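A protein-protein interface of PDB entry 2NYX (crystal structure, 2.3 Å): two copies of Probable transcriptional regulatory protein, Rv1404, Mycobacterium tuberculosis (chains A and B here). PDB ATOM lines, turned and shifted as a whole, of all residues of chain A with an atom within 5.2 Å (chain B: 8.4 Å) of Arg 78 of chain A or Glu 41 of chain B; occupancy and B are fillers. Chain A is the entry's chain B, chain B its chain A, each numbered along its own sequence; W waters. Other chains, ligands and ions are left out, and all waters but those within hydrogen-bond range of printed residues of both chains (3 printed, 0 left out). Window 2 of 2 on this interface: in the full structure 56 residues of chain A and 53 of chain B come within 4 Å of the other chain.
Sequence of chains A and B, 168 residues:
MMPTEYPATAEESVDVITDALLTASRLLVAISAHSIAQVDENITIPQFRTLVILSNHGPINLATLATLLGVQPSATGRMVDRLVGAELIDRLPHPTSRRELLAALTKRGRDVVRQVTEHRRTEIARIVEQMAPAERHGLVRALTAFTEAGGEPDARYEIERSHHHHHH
The side-chain carboxylate of Glu 41 of chain B lies within salt-bridge range of the guanidinium group of Arg 82 of chain A, 3.9 Å away.
The side-chain carboxylate of Glu 41 of chain B lies within salt-bridge range of the guanidinium group of Arg 78 of chain A, 2.9 Å away.
The side-chain amide nitrogen (ND2) of Asn 42 of chain B lies close to the guanidinium group (NH2) of Arg 82 of chain A.
The backbone NH (N) of Asn 42 of chain B lies close to the side-chain carboxylate (OD1) of Asp 40 of chain B (3.2 Å).
N of Ile 43 of chain B is in hydrogen-bond range of OD1 of Asp 40 of chain B, at 3.4 Å.
The backbone carbonyl oxygen of Ser 74 of chain A sits at hydrogen-bond distance from the guanidinium group of Arg 78 of chain A, 3.3 Å away.
Among the printed residues, merely in contact across the chains: Thr 44 of chain A with Asn 42 of chain B, Thr 44 of chain A with Ile 43 of chain B and Ala 75 of chain A with Glu 41 of chain B.
Of the printed residues of chain B, Thr 44 of chain A touches Asn 42 and Ile 43.
No residue of chain B comes within 4 Å of Gly 77 of chain A.
Arg 78 of chain A touches just one residue of chain B: Glu 41.
Asp 81 of chain A touches none of the printed residues of chain B.
Val 39 of chain B touches none of the printed residues of chain A.
Of chain A, only Ala 75, Arg 78 and Arg 82 come within 4 Å of Glu 41 of chain B.
Of the printed residues of chain A, Asn 42 of chain B touches Thr 44 (3.8 Å) and Arg 82 (3.0 Å).
Printed residues of chain A within 4 Å of Ile 43 of chain B: Thr 44 (3.6 Å).
The nearest residue of chain B that does not touch Arg 78 of chain A is Asn 42 of chain B (5.9 Å).
The nearest printed residue of chain B that does not touch Thr 44 of chain A is Thr 44 of chain B (4.3 Å).
Of the 12 printed residues of chain B, 3 touch a printed residue of chain A.
Printed residues of chain B that touch a printed residue of chain A: Glu 41, Asn 42 and Ile 43.
Of the 12 printed residues of chain A, 4 touch a printed residue of chain B.
Hydrophobic or aromatic side chains of chain A within 4 Å of the printed part of chain B: Ala 75.
Among the printed residues, 6 pairs touch across the chains.
Among the printed residues, Asp or Glu carboxylates within 4 Å of a Lys or Arg side-chain nitrogen of the other chain: Arg 78 of chain A with Glu 41 of chain B and Arg 82 of chain A with Glu 41 of chain B.
1 position is printed for both chains.
Of the 6 pairs that touch across the chains among the printed residues, none has its exchanged pair printed and touching as well.
Water W2 lies within hydrogen-bond range of the side-chain carboxylate (OE2) of Glu 41 of chain B, the guanidinium group (NH1) of Arg 82 of chain A, the backbone carbonyl oxygen (O) of Ala 75 of chain A and the backbone NH (N) of Met 79 of chain A.
Water W1 lies within hydrogen-bond range of N of Gln 72 of chain A (2.7 Å) and NE2 of Gln 38 of chain B (2.9 Å).
Water W3 lies within hydrogen-bond range of the guanidinium group (NH2) of Arg 82 of chain A (3.3 Å), the guanidinium group (NH1) of Arg 78 of chain A (3.3 Å), the side-chain amide oxygen (OD1) of Asn 42 of chain B (3.5 Å) and the side-chain carboxylate (OE2) of Glu 41 of chain B (3.5 Å).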
ATOM      1  N   THR A  44     -17.828   7.945   7.368  1.00  0.00           N
ATOM      2  CA  THR A  44     -18.528   7.048   8.285  1.00  0.00           C
ATOM      3  C   THR A  44     -17.601   5.933   8.751  1.00  0.00           C
ATOM      4  O   THR A  44     -16.564   5.686   8.144  1.00  0.00           O
ATOM      5  CB  THR A  44     -19.799   6.407   7.651  1.00  0.00           C
ATOM      6  OG1 THR A  44     -19.422   5.398   6.700  1.00  0.00           O
ATOM      7  CG2 THR A  44     -20.691   7.452   6.987  1.00  0.00           C
ATOM      8  N   GLN A  72     -23.980  -6.102   3.657  1.00  0.00           N
ATOM      9  CA  GLN A  72     -24.702  -6.469   2.441  1.00  0.00           C
ATOM     10  C   GLN A  72     -24.018  -5.878   1.195  1.00  0.00           C
ATOM     11  O   GLN A  72     -23.596  -4.728   1.225  1.00  0.00           O
ATOM     12  CB  GLN A  72     -26.168  -6.018   2.567  1.00  0.00           C
ATOM     13  CG  GLN A  72     -26.793  -5.412   1.302  1.00  0.00           C
ATOM     14  CD  GLN A  72     -28.137  -4.719   1.562  1.00  0.00           C
ATOM     15  OE1 GLN A  72     -28.308  -4.002   2.563  1.00  0.00           O
ATOM     16  NE2 GLN A  72     -29.099  -4.933   0.657  1.00  0.00           N
ATOM     17  N   PRO A  73     -23.886  -6.671   0.108  1.00  0.00           N
ATOM     18  CA  PRO A  73     -23.184  -6.228  -1.110  1.00  0.00           C
ATOM     19  C   PRO A  73     -23.703  -4.939  -1.772  1.00  0.00           C
ATOM     20  O   PRO A  73     -22.891  -4.124  -2.227  1.00  0.00           O
ATOM     21  CB  PRO A  73     -23.308  -7.427  -2.062  1.00  0.00           C
ATOM     22  CG  PRO A  73     -24.381  -8.280  -1.497  1.00  0.00           C
ATOM     23  CD  PRO A  73     -24.378  -8.055  -0.021  1.00  0.00           C
ATOM     24  N   SER A  74     -25.023  -4.754  -1.834  1.00  0.00           N
ATOM     25  CA  SER A  74     -25.594  -3.553  -2.462  1.00  0.00           C
ATOM     26  C   SER A  74     -25.066  -2.292  -1.787  1.00  0.00           C
ATOM     27  O   SER A  74     -24.622  -1.349  -2.458  1.00  0.00           O
ATOM     28  CB  SER A  74     -27.118  -3.563  -2.394  1.00  0.00           C
ATOM     29  OG  SER A  74     -27.657  -4.586  -3.205  1.00  0.00           O
ATOM     30  N   ALA A  75     -25.117  -2.307  -0.452  1.00  0.00           N
ATOM     31  CA  ALA A  75     -24.627  -1.224   0.383  1.00  0.00           C
ATOM     32  C   ALA A  75     -23.121  -1.059   0.250  1.00  0.00           C
ATOM     33  O   ALA A  75     -22.641   0.060   0.143  1.00  0.00           O
ATOM     34  CB  ALA A  75     -25.014  -1.453   1.834  1.00  0.00           C
ATOM     35  N   THR A  76     -22.382  -2.164   0.256  1.00  0.00           N
ATOM     36  CA  THR A  76     -20.934  -2.127   0.017  1.00  0.00           C
ATOM     37  C   THR A  76     -20.625  -1.418  -1.311  1.00  0.00           C
ATOM     38  O   THR A  76     -19.803  -0.502  -1.369  1.00  0.00           O
ATOM     39  CB  THR A  76     -20.317  -3.550  -0.007  1.00  0.00           C
ATOM     40  OG1 THR A  76     -20.770  -4.293   1.122  1.00  0.00           O
ATOM     41  CG2 THR A  76     -18.804  -3.484   0.037  1.00  0.00           C
ATOM     42  N   GLY A  77     -21.302  -1.844  -2.368  1.00  0.00           N
ATOM     43  CA  GLY A  77     -21.122  -1.255  -3.679  1.00  0.00           C
ATOM     44  C   GLY A  77     -21.320   0.241  -3.658  1.00  0.00           C
ATOM     45  O   GLY A  77     -20.528   0.970  -4.237  1.00  0.00           O
ATOM     46  N   ARG A  78     -22.383   0.686  -2.985  1.00  0.00           N
ATOM     47  CA  ARG A  78     -22.687   2.108  -2.830  1.00  0.00           C
ATOM     48  C   ARG A  78     -21.620   2.898  -2.073  1.00  0.00           C
ATOM     49  O   ARG A  78     -21.274   4.003  -2.483  1.00  0.00           O
ATOM     50  CB  ARG A  78     -24.055   2.309  -2.183  1.00  0.00           C
ATOM     51  CG  ARG A  78     -25.199   2.377  -3.180  1.00  0.00           C
ATOM     52  CD  ARG A  78     -26.542   2.357  -2.490  1.00  0.00           C
ATOM     53  NE  ARG A  78     -26.884   1.021  -2.004  1.00  0.00           N
ATOM     54  CZ  ARG A  78     -27.812   0.761  -1.092  1.00  0.00           C
ATOM     55  NH1 ARG A  78     -28.515   1.743  -0.544  1.00  0.00           N
ATOM     56  NH2 ARG A  78     -28.042  -0.489  -0.720  1.00  0.00           N
ATOM     57  N   MET A  79     -21.094   2.341  -0.984  1.00  0.00           N
ATOM     58  CA  MET A  79     -20.056   3.045  -0.222  1.00  0.00           C
ATOM     59  C   MET A  79     -18.682   3.053  -0.896  1.00  0.00           C
ATOM     60  O   MET A  79     -17.886   3.948  -0.651  1.00  0.00           O
ATOM     61  CB  MET A  79     -19.986   2.602   1.249  1.00  0.00           C
ATOM     62  CG  MET A  79     -19.459   1.210   1.510  1.00  0.00           C
ATOM     63  SD  MET A  79     -19.631   0.674   3.436  1.00  0.00           S
ATOM     64  CE  MET A  79     -21.617   0.839   3.684  1.00  0.00           C
ATOM     65  N   VAL A  80     -18.413   2.071  -1.749  1.00  0.00           N
ATOM     66  CA  VAL A  80     -17.205   2.091  -2.578  1.00  0.00           C
ATOM     67  C   VAL A  80     -17.340   3.198  -3.631  1.00  0.00           C
ATOM     68  O   VAL A  80     -16.400   3.965  -3.843  1.00  0.00           O
ATOM     69  CB  VAL A  80     -16.899   0.711  -3.228  1.00  0.00           C
ATOM     70  CG1 VAL A  80     -15.735   0.801  -4.209  1.00  0.00           C
ATOM     71  CG2 VAL A  80     -16.567  -0.301  -2.170  1.00  0.00           C
ATOM     72  N   ASP A  81     -18.510   3.299  -4.262  1.00  0.00           N
ATOM     73  CA  ASP A  81     -18.789   4.393  -5.195  1.00  0.00           C
ATOM     74  C   ASP A  81     -18.493   5.765  -4.583  1.00  0.00           C
ATOM     75  O   ASP A  81     -17.869   6.616  -5.225  1.00  0.00           O
ATOM     76  CB  ASP A  81     -20.245   4.360  -5.670  1.00  0.00           C
ATOM     77  CG  ASP A  81     -20.539   3.202  -6.603  1.00  0.00           C
ATOM     78  OD1 ASP A  81     -19.612   2.724  -7.297  1.00  0.00           O
ATOM     79  OD2 ASP A  81     -21.718   2.777  -6.651  1.00  0.00           O
ATOM     80  N   ARG A  82     -18.949   5.967  -3.350  1.00  0.00           N
ATOM     81  CA  ARG A  82     -18.755   7.219  -2.629  1.00  0.00           C
ATOM     82  C   ARG A  82     -17.282   7.479  -2.365  1.00  0.00           C
ATOM     83  O   ARG A  82     -16.790   8.589  -2.558  1.00  0.00           O
ATOM     84  CB  ARG A  82     -19.527   7.207  -1.304  1.00  0.00           C
ATOM     85  CG  ARG A  82     -21.019   7.356  -1.472  1.00  0.00           C
ATOM     86  CD  ARG A  82     -21.734   7.591  -0.144  1.00  0.00           C
ATOM     87  NE  ARG A  82     -23.165   7.294  -0.270  1.00  0.00           N
ATOM     88  CZ  ARG A  82     -23.739   6.148   0.103  1.00  0.00           C
ATOM     89  NH1 ARG A  82     -23.011   5.175   0.654  1.00  0.00           N
ATOM     90  NH2 ARG A  82     -25.045   5.974  -0.071  1.00  0.00           N
ATOM     91  N   ALA B  33     -18.608  -1.208  12.530  1.00  0.00           N
ATOM     92  CA  ALA B  33     -18.870  -0.988  11.111  1.00  0.00           C
ATOM     93  C   ALA B  33     -19.883  -1.993  10.564  1.00  0.00           C
ATOM     94  O   ALA B  33     -20.862  -1.614   9.911  1.00  0.00           O
ATOM     95  CB  ALA B  33     -17.585  -1.048  10.322  1.00  0.00           C
ATOM     96  N   SER B  35     -22.069  -3.577  12.383  1.00  0.00           N
ATOM     97  CA  SER B  35     -23.344  -3.335  13.054  1.00  0.00           C
ATOM     98  C   SER B  35     -24.079  -2.111  12.522  1.00  0.00           C
ATOM     99  O   SER B  35     -25.277  -2.176  12.234  1.00  0.00           O
ATOM    100  CB  SER B  35     -23.128  -3.189  14.555  1.00  0.00           C
ATOM    101  OG  SER B  35     -22.657  -4.399  15.107  1.00  0.00           O
ATOM    102  N   ILE B  36     -23.367  -1.000  12.388  1.00  0.00           N
ATOM    103  CA  ILE B  36     -23.979   0.236  11.931  1.00  0.00           C
ATOM    104  C   ILE B  36     -24.510   0.107  10.495  1.00  0.00           C
ATOM    105  O   ILE B  36     -25.664   0.444  10.229  1.00  0.00           O
ATOM    106  CB  ILE B  36     -23.006   1.419  12.076  1.00  0.00           C
ATOM    107  CG1 ILE B  36     -22.640   1.607  13.548  1.00  0.00           C
ATOM    108  CG2 ILE B  36     -23.626   2.696  11.546  1.00  0.00           C
ATOM    109  CD1 ILE B  36     -21.350   2.375  13.762  1.00  0.00           C
ATOM    110  N   ALA B  37     -23.668  -0.406   9.597  1.00  0.00           N
ATOM    111  CA  ALA B  37     -23.986  -0.538   8.178  1.00  0.00           C
ATOM    112  C   ALA B  37     -25.173  -1.454   7.902  1.00  0.00           C
ATOM    113  O   ALA B  37     -25.953  -1.205   6.988  1.00  0.00           O
ATOM    114  CB  ALA B  37     -22.771  -1.027   7.426  1.00  0.00           C
ATOM    115  N   GLN B  38     -25.291  -2.519   8.685  1.00  0.00           N
ATOM    116  CA  GLN B  38     -26.395  -3.462   8.582  1.00  0.00           C
ATOM    117  C   GLN B  38     -27.742  -2.793   8.849  1.00  0.00           C
ATOM    118  O   GLN B  38     -28.756  -3.177   8.266  1.00  0.00           O
ATOM    119  CB  GLN B  38     -26.198  -4.581   9.597  1.00  0.00           C
ATOM    120  CG  GLN B  38     -26.746  -5.917   9.144  1.00  0.00           C
ATOM    121  CD  GLN B  38     -25.735  -6.684   8.329  1.00  0.00           C
ATOM    122  OE1 GLN B  38     -24.538  -6.602   8.594  1.00  0.00           O
ATOM    123  NE2 GLN B  38     -26.205  -7.428   7.328  1.00  0.00           N
ATOM    124  N   VAL B  39     -27.733  -1.806   9.747  1.00  0.00           N
ATOM    125  CA  VAL B  39     -28.934  -1.098  10.168  1.00  0.00           C
ATOM    126  C   VAL B  39     -29.141   0.191   9.371  1.00  0.00           C
ATOM    127  O   VAL B  39     -30.254   0.463   8.937  1.00  0.00           O
ATOM    128  CB  VAL B  39     -28.912  -0.811  11.692  1.00  0.00           C
ATOM    129  CG1 VAL B  39     -30.144  -0.024  12.123  1.00  0.00           C
ATOM    130  CG2 VAL B  39     -28.824  -2.120  12.482  1.00  0.00           C
ATOM    131  N   ASP B  40     -28.076   0.970   9.171  1.00  0.00           N
ATOM    132  CA  ASP B  40     -28.137   2.235   8.424  1.00  0.00           C
ATOM    133  C   ASP B  40     -26.795   2.557   7.753  1.00  0.00           C
ATOM    134  O   ASP B  40     -25.830   2.977   8.399  1.00  0.00           O
ATOM    135  CB  ASP B  40     -28.569   3.378   9.353  1.00  0.00           C
ATOM    136  CG  ASP B  40     -29.049   4.617   8.592  1.00  0.00           C
ATOM    137  OD1 ASP B  40     -28.589   4.877   7.456  1.00  0.00           O
ATOM    138  OD2 ASP B  40     -29.891   5.350   9.152  1.00  0.00           O
ATOM    139  N   GLU B  41     -26.748   2.377   6.442  1.00  0.00           N
ATOM    140  CA  GLU B  41     -25.488   2.476   5.705  1.00  0.00           C
ATOM    141  C   GLU B  41     -24.988   3.916   5.557  1.00  0.00           C
ATOM    142  O   GLU B  41     -23.843   4.141   5.166  1.00  0.00           O
ATOM    143  CB  GLU B  41     -25.628   1.826   4.327  1.00  0.00           C
ATOM    144  CG  GLU B  41     -26.482   2.636   3.362  1.00  0.00           C
ATOM    145  CD  GLU B  41     -26.671   1.942   2.049  1.00  0.00           C
ATOM    146  OE1 GLU B  41     -27.402   0.933   2.026  1.00  0.00           O
ATOM    147  OE2 GLU B  41     -26.098   2.408   1.040  1.00  0.00           O
ATOM    148  N   ASN B  42     -25.853   4.878   5.869  1.00  0.00           N
ATOM    149  CA  ASN B  42     -25.546   6.290   5.668  1.00  0.00           C
ATOM    150  C   ASN B  42     -25.197   7.059   6.941  1.00  0.00           C
ATOM    151  O   ASN B  42     -24.438   8.028   6.889  1.00  0.00           O
ATOM    152  CB  ASN B  42     -26.711   6.986   4.965  1.00  0.00           C
ATOM    153  CG  ASN B  42     -26.954   6.454   3.571  1.00  0.00           C
ATOM    154  OD1 ASN B  42     -28.100   6.252   3.176  1.00  0.00           O
ATOM    155  ND2 ASN B  42     -25.881   6.224   2.814  1.00  0.00           N
ATOM    156  N   ILE B  43     -25.759   6.644   8.070  1.00  0.00           N
ATOM    157  CA  ILE B  43     -25.626   7.403   9.309  1.00  0.00           C
ATOM    158  C   ILE B  43     -24.150   7.690   9.621  1.00  0.00           C
ATOM    159  O   ILE B  43     -23.283   6.825   9.425  1.00  0.00           O
ATOM    160  CB  ILE B  43     -26.366   6.695  10.480  1.00  0.00           C
ATOM    161  CG1 ILE B  43     -26.609   7.657  11.650  1.00  0.00           C
ATOM    162  CG2 ILE B  43     -25.652   5.422  10.908  1.00  0.00           C
ATOM    163  CD1 ILE B  43     -27.570   7.128  12.698  1.00  0.00           C
ATOM    164  N   THR B  44     -23.868   8.910  10.077  1.00  0.00           N
ATOM    165  CA  THR B  44     -22.492   9.338  10.355  1.00  0.00           C
ATOM    166  C   THR B  44     -22.080   9.076  11.803  1.00  0.00           C
ATOM    167  O   THR B  44     -22.869   8.561  12.595  1.00  0.00           O
ATOM    168  CB  THR B  44     -22.292  10.827  10.035  1.00  0.00           C
ATOM    169  OG1 THR B  44     -23.221  11.602  10.795  1.00  0.00           O
ATOM    170  CG2 THR B  44     -22.511  11.094   8.552  1.00  0.00           C
ATOM    171  N   GLN B  47     -23.926  11.722  14.109  1.00  0.00           N
ATOM    172  CA  GLN B  47     -25.337  11.349  14.123  1.00  0.00           C
ATOM    173  C   GLN B  47     -25.623  10.164  15.043  1.00  0.00           C
ATOM    174  O   GLN B  47     -26.500  10.237  15.908  1.00  0.00           O
ATOM    175  CB  GLN B  47     -25.835  11.044  12.714  1.00  0.00           C
ATOM    176  CG  GLN B  47     -26.043  12.266  11.845  1.00  0.00           C
ATOM    177  CD  GLN B  47     -26.474  11.912  10.438  1.00  0.00           C
ATOM    178  OE1 GLN B  47     -26.573  10.743  10.081  1.00  0.00           O
ATOM    179  NE2 GLN B  47     -26.738  12.926   9.630  1.00  0.00           N
HETATM  180  O   HOH W   1     -25.727  -5.154   5.543  1.00  0.00           O
HETATM  181  O   HOH W   2     -23.415   2.510   1.458  1.00  0.00           O
HETATM  182  O   HOH W   3     -28.172   4.980  -0.045  1.00  0.00           O
